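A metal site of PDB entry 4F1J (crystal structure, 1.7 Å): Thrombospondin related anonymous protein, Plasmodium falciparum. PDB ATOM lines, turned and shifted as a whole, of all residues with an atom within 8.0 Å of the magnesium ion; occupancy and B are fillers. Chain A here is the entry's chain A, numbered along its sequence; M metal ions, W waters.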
ATOM      1  N   ASP A  15     -25.813  -1.351   9.588  1.00  0.00           N
ATOM      2  CA  ASP A  15     -25.675   0.095   9.738  1.00  0.00           C
ATOM      3  C   ASP A  15     -24.578   0.351  10.774  1.00  0.00           C
ATOM      4  O   ASP A  15     -24.620  -0.218  11.870  1.00  0.00           O
ATOM      5  CB  ASP A  15     -27.029   0.606  10.178  1.00  0.00           C
ATOM      6  CG  ASP A  15     -27.094   2.105  10.478  1.00  0.00           C
ATOM      7  OD1 ASP A  15     -26.100   2.741  10.886  1.00  0.00           O
ATOM      8  OD2 ASP A  15     -28.242   2.593  10.382  1.00  0.00           O
ATOM      9  N   CYS A  16     -23.582   1.171  10.420  1.00  0.00           N
ATOM     10  CA  CYS A  16     -22.491   1.521  11.374  1.00  0.00           C
ATOM     11  C   CYS A  16     -22.372   3.047  11.546  1.00  0.00           C
ATOM     12  O   CYS A  16     -21.295   3.568  11.878  1.00  0.00           O
ATOM     13  CB  CYS A  16     -21.169   0.885  10.935  1.00  0.00           C
ATOM     14  SG  CYS A  16     -20.545   1.425   9.335  1.00  0.00           S
ATOM     15  N   SER A  17     -23.500   3.710  11.386  1.00  0.00           N
ATOM     16  CA  SER A  17     -23.599   5.179  11.414  1.00  0.00           C
ATOM     17  C   SER A  17     -23.202   5.760  12.784  1.00  0.00           C
ATOM     18  O   SER A  17     -23.340   5.101  13.820  1.00  0.00           O
ATOM     19  CB  SER A  17     -25.010   5.651  11.061  1.00  0.00           C
ATOM     20  OG  SER A  17     -25.995   5.149  11.945  1.00  0.00           O
ATOM     21  N   GLY A  18     -22.744   7.010  12.755  1.00  0.00           N
ATOM     22  CA  GLY A  18     -22.279   7.675  13.997  1.00  0.00           C
ATOM     23  C   GLY A  18     -23.311   7.808  15.098  1.00  0.00           C
ATOM     24  O   GLY A  18     -22.979   7.783  16.293  1.00  0.00           O
ATOM     25  N   SER A  19     -24.586   7.868  14.715  1.00  0.00           N
ATOM     26  CA  SER A  19     -25.705   7.973  15.654  1.00  0.00           C
ATOM     27  C   SER A  19     -25.745   6.867  16.702  1.00  0.00           C
ATOM     28  O   SER A  19     -26.294   7.047  17.802  1.00  0.00           O
ATOM     29  CB  SER A  19     -27.007   7.902  14.883  1.00  0.00           C
ATOM     30  OG  SER A  19     -27.078   6.658  14.224  1.00  0.00           O
ATOM     31  N   ILE A  20     -25.166   5.735  16.347  1.00  0.00           N
ATOM     32  CA  ILE A  20     -25.148   4.546  17.213  1.00  0.00           C
ATOM     33  C   ILE A  20     -24.512   4.793  18.577  1.00  0.00           C
ATOM     34  O   ILE A  20     -25.017   4.303  19.584  1.00  0.00           O
ATOM     35  CB  ILE A  20     -24.432   3.377  16.519  1.00  0.00           C
ATOM     36  CG1 ILE A  20     -25.297   2.882  15.335  1.00  0.00           C
ATOM     37  CG2 ILE A  20     -24.131   2.221  17.519  1.00  0.00           C
ATOM     38  CD1 ILE A  20     -24.647   1.778  14.476  1.00  0.00           C
ATOM     39  N   ARG A  21     -23.433   5.564  18.568  1.00  0.00           N
ATOM     40  CA  ARG A  21     -22.550   5.781  19.706  1.00  0.00           C
ATOM     41  C   ARG A  21     -21.697   4.545  19.964  1.00  0.00           C
ATOM     42  O   ARG A  21     -22.171   3.391  19.937  1.00  0.00           O
ATOM     43  CB  ARG A  21     -23.295   6.209  20.968  1.00  0.00           C
ATOM     44  CG  ARG A  21     -24.233   7.394  20.796  1.00  0.00           C
ATOM     45  CD  ARG A  21     -23.485   8.646  20.432  1.00  0.00           C
ATOM     46  NE  ARG A  21     -24.349   9.805  20.201  1.00  0.00           N
ATOM     47  CZ  ARG A  21     -24.914  10.556  21.156  1.00  0.00           C
ATOM     48  NH1 ARG A  21     -24.741  10.297  22.450  1.00  0.00           N
ATOM     49  NH2 ARG A  21     -25.655  11.605  20.795  1.00  0.00           N
ATOM     50  N   PHE A  54     -22.393  -0.469   6.626  1.00  0.00           N
ATOM     51  CA  PHE A  54     -22.658   0.714   5.807  1.00  0.00           C
ATOM     52  C   PHE A  54     -22.935   1.934   6.673  1.00  0.00           C
ATOM     53  O   PHE A  54     -23.669   1.887   7.669  1.00  0.00           O
ATOM     54  CB  PHE A  54     -23.787   0.469   4.788  1.00  0.00           C
ATOM     55  CG  PHE A  54     -25.152   0.388   5.403  1.00  0.00           C
ATOM     56  CD1 PHE A  54     -25.637  -0.828   5.862  1.00  0.00           C
ATOM     57  CD2 PHE A  54     -25.961   1.502   5.529  1.00  0.00           C
ATOM     58  CE1 PHE A  54     -26.892  -0.926   6.431  1.00  0.00           C
ATOM     59  CE2 PHE A  54     -27.220   1.398   6.143  1.00  0.00           C
ATOM     60  CZ  PHE A  54     -27.662   0.197   6.594  1.00  0.00           C
ATOM     61  N   SER A  55     -22.272   3.027   6.300  1.00  0.00           N
ATOM     62  CA  SER A  55     -22.599   4.324   6.861  1.00  0.00           C
ATOM     63  C   SER A  55     -22.402   5.318   5.712  1.00  0.00           C
ATOM     64  O   SER A  55     -23.350   5.567   4.965  1.00  0.00           O
ATOM     65  CB  SER A  55     -21.787   4.605   8.139  1.00  0.00           C
ATOM     66  OG  SER A  55     -20.401   4.635   7.921  1.00  0.00           O
ATOM     67  N   GLY A  90     -20.338   8.202  10.653  1.00  0.00           N
ATOM     68  CA  GLY A  90     -20.840   8.527   9.333  1.00  0.00           C
ATOM     69  C   GLY A  90     -22.339   8.428   9.198  1.00  0.00           C
ATOM     70  O   GLY A  90     -23.050   8.266  10.186  1.00  0.00           O
ATOM     71  N   ARG A  91     -22.806   8.519   7.958  1.00  0.00           N
ATOM     72  CA  ARG A  91     -24.228   8.682   7.657  1.00  0.00           C
ATOM     73  C   ARG A  91     -24.902   7.332   7.394  1.00  0.00           C
ATOM     74  O   ARG A  91     -24.499   6.365   8.008  1.00  0.00           O
ATOM     75  CB  ARG A  91     -24.434   9.715   6.525  1.00  0.00           C
ATOM     76  CG  ARG A  91     -23.705   9.455   5.238  1.00  0.00           C
ATOM     77  CD  ARG A  91     -23.905  10.627   4.254  1.00  0.00           C
ATOM     78  NE  ARG A  91     -23.393  10.336   2.922  1.00  0.00           N
ATOM     79  CZ  ARG A  91     -24.013   9.585   2.010  1.00  0.00           C
ATOM     80  NH1 ARG A  91     -25.194   9.010   2.232  1.00  0.00           N
ATOM     81  NH2 ARG A  91     -23.453   9.405   0.823  1.00  0.00           N
ATOM     82  N   THR A  92     -25.951   7.282   6.578  1.00  0.00           N
ATOM     83  CA  THR A  92     -26.755   6.052   6.426  1.00  0.00           C
ATOM     84  C   THR A  92     -27.027   5.756   4.953  1.00  0.00           C
ATOM     85  O   THR A  92     -28.161   5.922   4.470  1.00  0.00           O
ATOM     86  CB  THR A  92     -28.074   6.167   7.214  1.00  0.00           C
ATOM     87  OG1 THR A  92     -27.792   6.659   8.547  1.00  0.00           O
ATOM     88  CG2 THR A  92     -28.824   4.837   7.287  1.00  0.00           C
ATOM     89  N   THR A 122     -30.551  -1.578  11.486  1.00  0.00           N
ATOM     90  CA  THR A 122     -30.394  -0.124  11.313  1.00  0.00           C
ATOM     91  C   THR A 122     -30.941   0.652  12.495  1.00  0.00           C
ATOM     92  O   THR A 122     -31.885   0.227  13.126  1.00  0.00           O
ATOM     93  CB  THR A 122     -31.064   0.359  10.001  1.00  0.00           C
ATOM     94  OG1 THR A 122     -30.677   1.724   9.693  1.00  0.00           O
ATOM     95  CG2 THR A 122     -32.583   0.203  10.049  1.00  0.00           C
ATOM     96  N   ASP A 123     -30.347   1.810  12.761  1.00  0.00           N
ATOM     97  CA  ASP A 123     -30.848   2.711  13.816  1.00  0.00           C
ATOM     98  C   ASP A 123     -31.338   4.057  13.241  1.00  0.00           C
ATOM     99  O   ASP A 123     -31.490   5.023  13.993  1.00  0.00           O
ATOM    100  CB  ASP A 123     -29.771   2.950  14.861  1.00  0.00           C
ATOM    101  CG  ASP A 123     -28.820   4.092  14.507  1.00  0.00           C
ATOM    102  OD1 ASP A 123     -28.528   4.321  13.289  1.00  0.00           O
ATOM    103  OD2 ASP A 123     -28.320   4.689  15.471  1.00  0.00           O
ATOM    104  N   GLY A 124     -31.538   4.109  11.936  1.00  0.00           N
ATOM    105  CA  GLY A 124     -31.892   5.363  11.272  1.00  0.00           C
ATOM    106  C   GLY A 124     -32.711   5.195  10.017  1.00  0.00           C
ATOM    107  O   GLY A 124     -33.186   4.093   9.685  1.00  0.00           O
ATOM    108  N   ILE A 125     -32.885   6.324   9.347  1.00  0.00           N
ATOM    109  CA  ILE A 125     -33.561   6.417   8.075  1.00  0.00           C
ATOM    110  C   ILE A 125     -32.496   6.570   6.971  1.00  0.00           C
ATOM    111  O   ILE A 125     -31.514   7.314   7.155  1.00  0.00           O
ATOM    112  CB  ILE A 125     -34.517   7.625   8.085  1.00  0.00           C
ATOM    113  CG1 ILE A 125     -35.592   7.452   9.172  1.00  0.00           C
ATOM    114  CG2 ILE A 125     -35.190   7.777   6.731  1.00  0.00           C
ATOM    115  CD1 ILE A 125     -36.132   8.753   9.678  1.00  0.00           C
ATOM    116  N   ASP A 127     -30.337   7.896   3.926  1.00  0.00           N
ATOM    117  CA  ASP A 127     -30.074   9.261   3.446  1.00  0.00           C
ATOM    118  C   ASP A 127     -30.875   9.576   2.198  1.00  0.00           C
ATOM    119  O   ASP A 127     -31.262  10.741   1.983  1.00  0.00           O
ATOM    120  CB  ASP A 127     -28.595   9.447   3.248  1.00  0.00           C
ATOM    121  CG  ASP A 127     -27.824   9.400   4.584  1.00  0.00           C
ATOM    122  OD1 ASP A 127     -28.319   9.834   5.648  1.00  0.00           O
ATOM    123  OD2 ASP A 127     -26.712   8.908   4.543  1.00  0.00           O
ATOM    124  N   ILE A 151     -33.639  -0.260  15.407  1.00  0.00           N
ATOM    125  CA  ILE A 151     -33.109  -0.083  16.751  1.00  0.00           C
ATOM    126  C   ILE A 151     -33.195   1.367  17.201  1.00  0.00           C
ATOM    127  O   ILE A 151     -32.731   2.255  16.509  1.00  0.00           O
ATOM    128  CB  ILE A 151     -31.632  -0.488  16.848  1.00  0.00           C
ATOM    129  CG1 ILE A 151     -31.419  -1.869  16.242  1.00  0.00           C
ATOM    130  CG2 ILE A 151     -31.192  -0.468  18.311  1.00  0.00           C
ATOM    131  CD1 ILE A 151     -29.985  -2.236  16.041  1.00  0.00           C
ATOM    132  N   GLY A 154     -34.350   6.595  16.437  1.00  0.00           N
ATOM    133  CA  GLY A 154     -34.075   7.309  15.198  1.00  0.00           C
ATOM    134  C   GLY A 154     -34.655   6.689  13.935  1.00  0.00           C
ATOM    135  O   GLY A 154     -34.518   7.282  12.860  1.00  0.00           O
ATOM    136  N   ILE A 155     -35.299   5.538  14.062  1.00  0.00           N
ATOM    137  CA  ILE A 155     -35.881   4.826  12.931  1.00  0.00           C
ATOM    138  C   ILE A 155     -37.224   5.446  12.551  1.00  0.00           C
ATOM    139  O   ILE A 155     -37.866   6.172  13.346  1.00  0.00           O
ATOM    140  CB  ILE A 155     -36.083   3.317  13.207  1.00  0.00           C
ATOM    141  CG1 ILE A 155     -36.950   3.086  14.461  1.00  0.00           C
ATOM    142  CG2 ILE A 155     -34.737   2.599  13.385  1.00  0.00           C
ATOM    143  CD1 ILE A 155     -37.394   1.619  14.642  1.00  0.00           C
ATOM    144  N   TRP A 181     -32.269  -0.187  22.406  1.00  0.00           N
ATOM    145  CA  TRP A 181     -30.899  -0.650  22.389  1.00  0.00           C
ATOM    146  C   TRP A 181     -30.650  -1.768  23.410  1.00  0.00           C
ATOM    147  O   TRP A 181     -30.070  -2.791  23.089  1.00  0.00           O
ATOM    148  CB  TRP A 181     -29.938   0.515  22.642  1.00  0.00           C
ATOM    149  CG  TRP A 181     -29.556   1.213  21.394  1.00  0.00           C
ATOM    150  CD1 TRP A 181     -29.948   2.450  20.992  1.00  0.00           C
ATOM    151  CD2 TRP A 181     -28.746   0.682  20.330  1.00  0.00           C
ATOM    152  NE1 TRP A 181     -29.415   2.735  19.766  1.00  0.00           N
ATOM    153  CE2 TRP A 181     -28.660   1.669  19.337  1.00  0.00           C
ATOM    154  CE3 TRP A 181     -28.075  -0.531  20.144  1.00  0.00           C
ATOM    155  CZ2 TRP A 181     -27.953   1.475  18.149  1.00  0.00           C
ATOM    156  CZ3 TRP A 181     -27.357  -0.724  18.984  1.00  0.00           C
ATOM    157  CH2 TRP A 181     -27.291   0.289  17.995  1.00  0.00           C
HETATM  158 MG    MG M   1     -27.939   6.087  12.406  1.00  0.00          MG
HETATM  159  O   HOH W   1     -29.623   7.028  13.025  1.00  0.00           O
HETATM  160  O   HOH W   2     -28.632   5.170  10.601  1.00  0.00           O
HETATM  161  O   HOH W   3     -27.492   7.819  11.576  1.00  0.00           O
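Thr 92 touches the magnesium ion (OG1 to MG, 3.9 Å). The nearest printed residue that does not touch the magnesium ion is Asp 15 (4.05 Å).
The magnesium ion is bound by water W3 (2.0 Å), water W1 (2.0 Å), OD1 of Asp 123 (2.1 Å), OG of Ser 19 (2.1 Å), water W2 (2.1 Å) and OG of Ser 17 (2.2 Å).
Water W2 lies within hydrogen-bond range of the side-chain carboxylate (OD2) of Asp 15 (2.6 Å), the side-chain hydroxyl (OG1) of Thr 92 (2.7 Å) and the backbone NH (N) of Gly 124 (3.4 Å).
OD2 of Asp 123 lies within hydrogen-bond range of N of Ile 20 (3.4 Å). The backbone NH of Ser 17 lies within hydrogen-bond range of the side-chain carboxylate of Asp 15 (2.8 Å). N of Asp 123 lies within hydrogen-bond range of OD2 of Asp 15 (3.3 Å). The side-chain carboxylate of Asp 127 sits at hydrogen-bond distance from the backbone NH of Thr 92.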
